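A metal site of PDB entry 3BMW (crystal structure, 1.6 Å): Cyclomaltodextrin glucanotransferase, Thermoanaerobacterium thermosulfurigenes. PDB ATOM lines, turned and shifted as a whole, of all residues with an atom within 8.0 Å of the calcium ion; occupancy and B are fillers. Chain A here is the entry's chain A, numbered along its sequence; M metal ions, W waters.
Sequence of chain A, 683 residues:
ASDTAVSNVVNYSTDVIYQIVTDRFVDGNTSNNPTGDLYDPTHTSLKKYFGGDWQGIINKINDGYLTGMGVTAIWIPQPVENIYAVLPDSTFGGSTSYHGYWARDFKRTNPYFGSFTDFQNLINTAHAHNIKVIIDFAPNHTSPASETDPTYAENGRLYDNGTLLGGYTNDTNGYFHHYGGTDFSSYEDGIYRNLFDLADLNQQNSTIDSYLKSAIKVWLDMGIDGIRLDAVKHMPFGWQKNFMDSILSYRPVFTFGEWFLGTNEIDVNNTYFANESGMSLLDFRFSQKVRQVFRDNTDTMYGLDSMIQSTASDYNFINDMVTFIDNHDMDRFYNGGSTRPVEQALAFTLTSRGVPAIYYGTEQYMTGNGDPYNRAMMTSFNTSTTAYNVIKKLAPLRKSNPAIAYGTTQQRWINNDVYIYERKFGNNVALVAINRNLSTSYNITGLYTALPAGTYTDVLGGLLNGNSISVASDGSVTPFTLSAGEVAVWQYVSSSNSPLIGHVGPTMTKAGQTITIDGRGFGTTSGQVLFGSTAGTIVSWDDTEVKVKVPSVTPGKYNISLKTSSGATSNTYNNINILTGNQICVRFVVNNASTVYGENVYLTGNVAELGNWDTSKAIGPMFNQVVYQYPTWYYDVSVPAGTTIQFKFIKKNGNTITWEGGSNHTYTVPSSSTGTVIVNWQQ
The side-chain amide oxygen (OD1) of Asn 194 sits close to the backbone NH (N) of Asp 200 (3.3 Å).
O of Asn 140 sits at hydrogen-bond distance from N of Leu 201, at 2.9 Å.
The backbone NH (N) of His 177 sits at hydrogen-bond distance from the backbone carbonyl oxygen (O) of Asp 200 (2.9 Å).
ND2 of Asn 140 is in hydrogen-bond range of ND1 of His 141, 3.1 Å away.
N of Asn 140 is in hydrogen-bond range of SD of Met 235 (3.6 Å).
A ring nitrogen (ND1) of His 234 lies within hydrogen-bond range of the backbone carbonyl oxygen (O) of Gly 190 (2.8 Å).
The calcium ion is bound by O of His 234 (2.3 Å), OD1 of Asn 140 (2.4 Å), water W1 (2.5 Å), OD2 of Asp 200 (2.5 Å), O of Ile 191 (2.5 Å), water W3 (2.5 Å), water W2 (2.5 Å) and OD1 of Asp 200 (2.5 Å).
The nearest printed residue that does not touch the calcium ion is Met 235 (4.5 Å).
Water W3 lies within hydrogen-bond range of the backbone carbonyl oxygen of Asn 140, the backbone carbonyl oxygen of Leu 201 and the side-chain amide nitrogen of Gln 203.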
ATOM      1  N   PRO A 139      -5.989  27.546 -31.869  1.00  0.00           N
ATOM      2  CA  PRO A 139      -6.231  28.120 -30.546  1.00  0.00           C
ATOM      3  C   PRO A 139      -5.490  27.420 -29.402  1.00  0.00           C
ATOM      4  O   PRO A 139      -5.694  27.776 -28.233  1.00  0.00           O
ATOM      5  CB  PRO A 139      -7.744  27.965 -30.388  1.00  0.00           C
ATOM      6  CG  PRO A 139      -8.040  26.693 -31.119  1.00  0.00           C
ATOM      7  CD  PRO A 139      -7.090  26.656 -32.295  1.00  0.00           C
ATOM      8  N   ASN A 140      -4.629  26.451 -29.702  1.00  0.00           N
ATOM      9  CA  ASN A 140      -3.829  25.815 -28.645  1.00  0.00           C
ATOM     10  C   ASN A 140      -2.756  26.727 -28.069  1.00  0.00           C
ATOM     11  O   ASN A 140      -2.346  26.583 -26.911  1.00  0.00           O
ATOM     12  CB  ASN A 140      -3.156  24.535 -29.160  1.00  0.00           C
ATOM     13  CG  ASN A 140      -2.356  23.824 -28.066  1.00  0.00           C
ATOM     14  OD1 ASN A 140      -2.925  23.324 -27.099  1.00  0.00           O
ATOM     15  ND2 ASN A 140      -1.033  23.797 -28.231  1.00  0.00           N
ATOM     16  N   HIS A 141      -2.284  27.671 -28.875  1.00  0.00           N
ATOM     17  CA  HIS A 141      -1.094  28.420 -28.479  1.00  0.00           C
ATOM     18  C   HIS A 141      -0.962  29.713 -29.260  1.00  0.00           C
ATOM     19  O   HIS A 141      -1.637  29.913 -30.281  1.00  0.00           O
ATOM     20  CB  HIS A 141       0.152  27.561 -28.747  1.00  0.00           C
ATOM     21  CG  HIS A 141       0.210  27.033 -30.136  1.00  0.00           C
ATOM     22  ND1 HIS A 141      -0.196  25.750 -30.463  1.00  0.00           N
ATOM     23  CD2 HIS A 141       0.580  27.617 -31.298  1.00  0.00           C
ATOM     24  CE1 HIS A 141      -0.063  25.569 -31.764  1.00  0.00           C
ATOM     25  NE2 HIS A 141       0.399  26.693 -32.298  1.00  0.00           N
ATOM     26  N   HIS A 177      -0.510  28.259 -19.693  1.00  0.00           N
ATOM     27  CA  HIS A 177      -0.069  27.195 -18.796  1.00  0.00           C
ATOM     28  C   HIS A 177       1.422  27.283 -18.514  1.00  0.00           C
ATOM     29  O   HIS A 177       2.212  27.578 -19.423  1.00  0.00           O
ATOM     30  CB  HIS A 177      -0.370  25.823 -19.391  1.00  0.00           C
ATOM     31  CG  HIS A 177      -1.830  25.501 -19.477  1.00  0.00           C
ATOM     32  ND1 HIS A 177      -2.397  24.999 -20.624  1.00  0.00           N
ATOM     33  CD2 HIS A 177      -2.818  25.592 -18.567  1.00  0.00           C
ATOM     34  CE1 HIS A 177      -3.698  24.804 -20.419  1.00  0.00           C
ATOM     35  NE2 HIS A 177      -3.971  25.151 -19.177  1.00  0.00           N
ATOM     36  N   GLU A 188      -3.253  13.587 -20.927  1.00  0.00           N
ATOM     37  CA  GLU A 188      -3.186  14.714 -19.991  1.00  0.00           C
ATOM     38  C   GLU A 188      -1.928  15.550 -20.184  1.00  0.00           C
ATOM     39  O   GLU A 188      -1.990  16.772 -20.250  1.00  0.00           O
ATOM     40  CB  GLU A 188      -3.243  14.206 -18.538  1.00  0.00           C
ATOM     41  CG  GLU A 188      -3.139  15.320 -17.498  1.00  0.00           C
ATOM     42  CD  GLU A 188      -3.283  14.827 -16.066  1.00  0.00           C
ATOM     43  OE1 GLU A 188      -3.447  13.615 -15.836  1.00  0.00           O
ATOM     44  OE2 GLU A 188      -3.250  15.691 -15.152  1.00  0.00           O
ATOM     45  N   ASP A 189      -0.787  14.882 -20.299  1.00  0.00           N
ATOM     46  CA  ASP A 189       0.500  15.547 -20.483  1.00  0.00           C
ATOM     47  C   ASP A 189       0.468  16.438 -21.731  1.00  0.00           C
ATOM     48  O   ASP A 189       0.948  17.580 -21.697  1.00  0.00           O
ATOM     49  CB  ASP A 189       1.616  14.514 -20.562  1.00  0.00           C
ATOM     50  CG  ASP A 189       3.004  15.130 -20.565  1.00  0.00           C
ATOM     51  OD1 ASP A 189       3.647  15.174 -19.491  1.00  0.00           O
ATOM     52  OD2 ASP A 189       3.441  15.552 -21.639  1.00  0.00           O
ATOM     53  N   GLY A 190      -0.114  15.920 -22.810  1.00  0.00           N
ATOM     54  CA  GLY A 190      -0.157  16.629 -24.090  1.00  0.00           C
ATOM     55  C   GLY A 190      -1.107  17.803 -24.131  1.00  0.00           C
ATOM     56  O   GLY A 190      -1.024  18.644 -25.023  1.00  0.00           O
ATOM     57  N   ILE A 191      -2.031  17.865 -23.173  1.00  0.00           N
ATOM     58  CA  ILE A 191      -3.038  18.924 -23.154  1.00  0.00           C
ATOM     59  C   ILE A 191      -2.597  20.135 -22.343  1.00  0.00           C
ATOM     60  O   ILE A 191      -2.761  21.273 -22.786  1.00  0.00           O
ATOM     61  CB  ILE A 191      -4.400  18.418 -22.605  1.00  0.00           C
ATOM     62  CG1 ILE A 191      -5.047  17.443 -23.600  1.00  0.00           C
ATOM     63  CG2 ILE A 191      -5.349  19.603 -22.310  1.00  0.00           C
ATOM     64  CD1 ILE A 191      -6.233  16.673 -23.038  1.00  0.00           C
ATOM     65  N   TYR A 192      -2.049  19.891 -21.157  1.00  0.00           N
ATOM     66  CA  TYR A 192      -1.792  20.969 -20.199  1.00  0.00           C
ATOM     67  C   TYR A 192      -0.354  21.481 -20.231  1.00  0.00           C
ATOM     68  O   TYR A 192      -0.068  22.541 -19.670  1.00  0.00           O
ATOM     69  CB  TYR A 192      -2.237  20.572 -18.789  1.00  0.00           C
ATOM     70  CG  TYR A 192      -3.734  20.388 -18.717  1.00  0.00           C
ATOM     71  CD1 TYR A 192      -4.582  21.486 -18.498  1.00  0.00           C
ATOM     72  CD2 TYR A 192      -4.314  19.142 -18.931  1.00  0.00           C
ATOM     73  CE1 TYR A 192      -5.968  21.329 -18.463  1.00  0.00           C
ATOM     74  CE2 TYR A 192      -5.700  18.971 -18.899  1.00  0.00           C
ATOM     75  CZ  TYR A 192      -6.519  20.079 -18.666  1.00  0.00           C
ATOM     76  OH  TYR A 192      -7.891  19.923 -18.641  1.00  0.00           O
ATOM     77  N   ARG A 193       0.545  20.748 -20.894  1.00  0.00           N
ATOM     78  CA  ARG A 193       1.923  21.198 -21.049  1.00  0.00           C
ATOM     79  C   ARG A 193       2.113  21.753 -22.471  1.00  0.00           C
ATOM     80  O   ARG A 193       1.284  21.535 -23.348  1.00  0.00           O
ATOM     81  CB  ARG A 193       2.907  20.075 -20.750  1.00  0.00           C
ATOM     82  CG  ARG A 193       2.730  19.448 -19.363  1.00  0.00           C
ATOM     83  CD  ARG A 193       3.923  18.557 -19.000  1.00  0.00           C
ATOM     84  NE  ARG A 193       3.632  17.683 -17.862  1.00  0.00           N
ATOM     85  CZ  ARG A 193       3.702  18.060 -16.585  1.00  0.00           C
ATOM     86  NH1 ARG A 193       3.419  17.180 -15.623  1.00  0.00           N
ATOM     87  NH2 ARG A 193       4.061  19.295 -16.264  1.00  0.00           N
ATOM     88  N   ASN A 194       3.207  22.498 -22.686  1.00  0.00           N
ATOM     89  CA  ASN A 194       3.427  23.155 -23.972  1.00  0.00           C
ATOM     90  C   ASN A 194       3.726  22.169 -25.085  1.00  0.00           C
ATOM     91  O   ASN A 194       4.493  21.220 -24.897  1.00  0.00           O
ATOM     92  CB  ASN A 194       4.610  24.126 -23.906  1.00  0.00           C
ATOM     93  CG  ASN A 194       4.407  25.272 -22.921  1.00  0.00           C
ATOM     94  OD1 ASN A 194       3.277  25.682 -22.623  1.00  0.00           O
ATOM     95  ND2 ASN A 194       5.510  25.826 -22.434  1.00  0.00           N
ATOM     96  N   LEU A 195       3.155  22.426 -26.262  1.00  0.00           N
ATOM     97  CA  LEU A 195       3.575  21.756 -27.486  1.00  0.00           C
ATOM     98  C   LEU A 195       4.870  22.422 -27.938  1.00  0.00           C
ATOM     99  O   LEU A 195       4.880  23.598 -28.320  1.00  0.00           O
ATOM    100  CB  LEU A 195       2.496  21.883 -28.568  1.00  0.00           C
ATOM    101  CG  LEU A 195       2.795  21.297 -29.965  1.00  0.00           C
ATOM    102  CD1 LEU A 195       3.115  19.799 -29.883  1.00  0.00           C
ATOM    103  CD2 LEU A 195       1.636  21.556 -30.922  1.00  0.00           C
ATOM    104  N   LEU A 198       5.896  26.312 -27.710  1.00  0.00           N
ATOM    105  CA  LEU A 198       4.762  27.204 -27.996  1.00  0.00           C
ATOM    106  C   LEU A 198       4.020  27.526 -26.705  1.00  0.00           C
ATOM    107  O   LEU A 198       3.659  26.621 -25.957  1.00  0.00           O
ATOM    108  CB  LEU A 198       3.825  26.554 -29.023  1.00  0.00           C
ATOM    109  CG  LEU A 198       4.460  26.176 -30.367  1.00  0.00           C
ATOM    110  CD1 LEU A 198       3.540  25.222 -31.120  1.00  0.00           C
ATOM    111  CD2 LEU A 198       4.791  27.400 -31.222  1.00  0.00           C
ATOM    112  N   ALA A 199       3.816  28.828 -26.457  1.00  0.00           N
ATOM    113  CA  ALA A 199       3.127  29.283 -25.239  1.00  0.00           C
ATOM    114  C   ALA A 199       1.697  28.729 -25.214  1.00  0.00           C
ATOM    115  O   ALA A 199       0.859  29.145 -26.028  1.00  0.00           O
ATOM    116  CB  ALA A 199       3.127  30.803 -25.164  1.00  0.00           C
ATOM    117  N   ASP A 200       1.431  27.812 -24.286  1.00  0.00           N
ATOM    118  CA  ASP A 200       0.148  27.083 -24.255  1.00  0.00           C
ATOM    119  C   ASP A 200      -0.960  27.954 -23.676  1.00  0.00           C
ATOM    120  O   ASP A 200      -0.893  28.379 -22.528  1.00  0.00           O
ATOM    121  CB  ASP A 200       0.284  25.790 -23.450  1.00  0.00           C
ATOM    122  CG  ASP A 200      -0.703  24.719 -23.899  1.00  0.00           C
ATOM    123  OD1 ASP A 200      -0.727  24.375 -25.113  1.00  0.00           O
ATOM    124  OD2 ASP A 200      -1.456  24.211 -23.050  1.00  0.00           O
ATOM    125  N   LEU A 201      -1.990  28.208 -24.485  1.00  0.00           N
ATOM    126  CA  LEU A 201      -3.119  29.007 -24.025  1.00  0.00           C
ATOM    127  C   LEU A 201      -3.940  28.268 -22.970  1.00  0.00           C
ATOM    128  O   LEU A 201      -4.148  27.061 -23.072  1.00  0.00           O
ATOM    129  CB  LEU A 201      -4.000  29.436 -25.201  1.00  0.00           C
ATOM    130  CG  LEU A 201      -3.404  30.622 -25.971  1.00  0.00           C
ATOM    131  CD1 LEU A 201      -4.067  30.799 -27.341  1.00  0.00           C
ATOM    132  CD2 LEU A 201      -3.507  31.911 -25.162  1.00  0.00           C
ATOM    133  N   ASN A 202      -4.375  29.006 -21.952  1.00  0.00           N
ATOM    134  CA  ASN A 202      -5.274  28.469 -20.940  1.00  0.00           C
ATOM    135  C   ASN A 202      -6.716  28.781 -21.311  1.00  0.00           C
ATOM    136  O   ASN A 202      -7.255  29.826 -20.925  1.00  0.00           O
ATOM    137  CB  ASN A 202      -4.941  29.077 -19.571  1.00  0.00           C
ATOM    138  CG  ASN A 202      -5.858  28.562 -18.467  1.00  0.00           C
ATOM    139  OD1 ASN A 202      -6.682  27.667 -18.682  1.00  0.00           O
ATOM    140  ND2 ASN A 202      -5.722  29.142 -17.279  1.00  0.00           N
ATOM    141  N   GLN A 203      -7.345  27.881 -22.056  1.00  0.00           N
ATOM    142  CA  GLN A 203      -8.715  28.082 -22.519  1.00  0.00           C
ATOM    143  C   GLN A 203      -9.741  28.073 -21.383  1.00  0.00           C
ATOM    144  O   GLN A 203     -10.878  28.505 -21.578  1.00  0.00           O
ATOM    145  CB  GLN A 203      -9.128  27.038 -23.566  1.00  0.00           C
ATOM    146  CG  GLN A 203      -8.302  27.043 -24.863  1.00  0.00           C
ATOM    147  CD  GLN A 203      -7.063  26.169 -24.780  1.00  0.00           C
ATOM    148  OE1 GLN A 203      -6.904  25.392 -23.829  1.00  0.00           O
ATOM    149  NE2 GLN A 203      -6.172  26.297 -25.761  1.00  0.00           N
ATOM    150  N   ALA A 231      -3.952  21.016 -33.921  1.00  0.00           N
ATOM    151  CA  ALA A 231      -3.455  20.411 -32.685  1.00  0.00           C
ATOM    152  C   ALA A 231      -4.555  20.057 -31.674  1.00  0.00           C
ATOM    153  O   ALA A 231      -4.436  20.351 -30.475  1.00  0.00           O
ATOM    154  CB  ALA A 231      -2.391  21.337 -32.047  1.00  0.00           C
ATOM    155  N   LYS A 233      -5.450  17.285 -30.356  1.00  0.00           N
ATOM    156  CA  LYS A 233      -5.063  16.374 -29.280  1.00  0.00           C
ATOM    157  C   LYS A 233      -4.437  17.119 -28.092  1.00  0.00           C
ATOM    158  O   LYS A 233      -4.229  16.532 -27.030  1.00  0.00           O
ATOM    159  CB  LYS A 233      -4.136  15.252 -29.793  1.00  0.00           C
ATOM    160  CG  LYS A 233      -2.724  15.651 -30.125  1.00  0.00           C
ATOM    161  CD  LYS A 233      -1.975  14.506 -30.842  1.00  0.00           C
ATOM    162  CE  LYS A 233      -1.469  13.459 -29.878  1.00  0.00           C
ATOM    163  NZ  LYS A 233      -0.500  12.533 -30.568  1.00  0.00           N
ATOM    164  N   HIS A 234      -4.184  18.417 -28.269  1.00  0.00           N
ATOM    165  CA  HIS A 234      -3.460  19.236 -27.274  1.00  0.00           C
ATOM    166  C   HIS A 234      -4.332  20.213 -26.481  1.00  0.00           C
ATOM    167  O   HIS A 234      -3.822  21.020 -25.671  1.00  0.00           O
ATOM    168  CB  HIS A 234      -2.286  19.947 -27.947  1.00  0.00           C
ATOM    169  CG  HIS A 234      -1.292  19.001 -28.532  1.00  0.00           C
ATOM    170  ND1 HIS A 234      -0.491  18.200 -27.746  1.00  0.00           N
ATOM    171  CD2 HIS A 234      -1.013  18.664 -29.815  1.00  0.00           C
ATOM    172  CE1 HIS A 234       0.263  17.449 -28.522  1.00  0.00           C
ATOM    173  NE2 HIS A 234      -0.034  17.703 -29.782  1.00  0.00           N
ATOM    174  N   MET A 235      -5.643  20.137 -26.723  1.00  0.00           N
ATOM    175  CA  MET A 235      -6.610  20.922 -25.965  1.00  0.00           C
ATOM    176  C   MET A 235      -7.658  19.984 -25.368  1.00  0.00           C
ATOM    177  O   MET A 235      -7.875  18.885 -25.898  1.00  0.00           O
ATOM    178  CB  MET A 235      -7.286  21.961 -26.872  1.00  0.00           C
ATOM    179  CG  MET A 235      -6.328  23.018 -27.412  1.00  0.00           C
ATOM    180  SD  MET A 235      -7.071  24.069 -28.675  1.00  0.00           S
ATOM    181  CE  MET A 235      -6.981  22.994 -30.104  1.00  0.00           C
ATOM    182  N   PRO A 236      -8.313  20.401 -24.262  1.00  0.00           N
ATOM    183  CA  PRO A 236      -9.288  19.513 -23.642  1.00  0.00           C
ATOM    184  C   PRO A 236     -10.447  19.207 -24.586  1.00  0.00           C
ATOM    185  O   PRO A 236     -10.909  20.096 -25.300  1.00  0.00           O
ATOM    186  CB  PRO A 236      -9.809  20.318 -22.447  1.00  0.00           C
ATOM    187  CG  PRO A 236      -8.701  21.308 -22.157  1.00  0.00           C
ATOM    188  CD  PRO A 236      -8.197  21.680 -23.535  1.00  0.00           C
HETATM  189 CA    CA M   1      -2.741  22.862 -24.731  1.00  0.00          CA
HETATM  190  O   HOH W   1      -0.768  21.471 -25.191  1.00  0.00           O
HETATM  191  O   HOH W   2      -4.987  23.159 -23.597  1.00  0.00           O
HETATM  192  O   HOH W   3      -3.596  25.206 -25.031  1.00  0.00           O
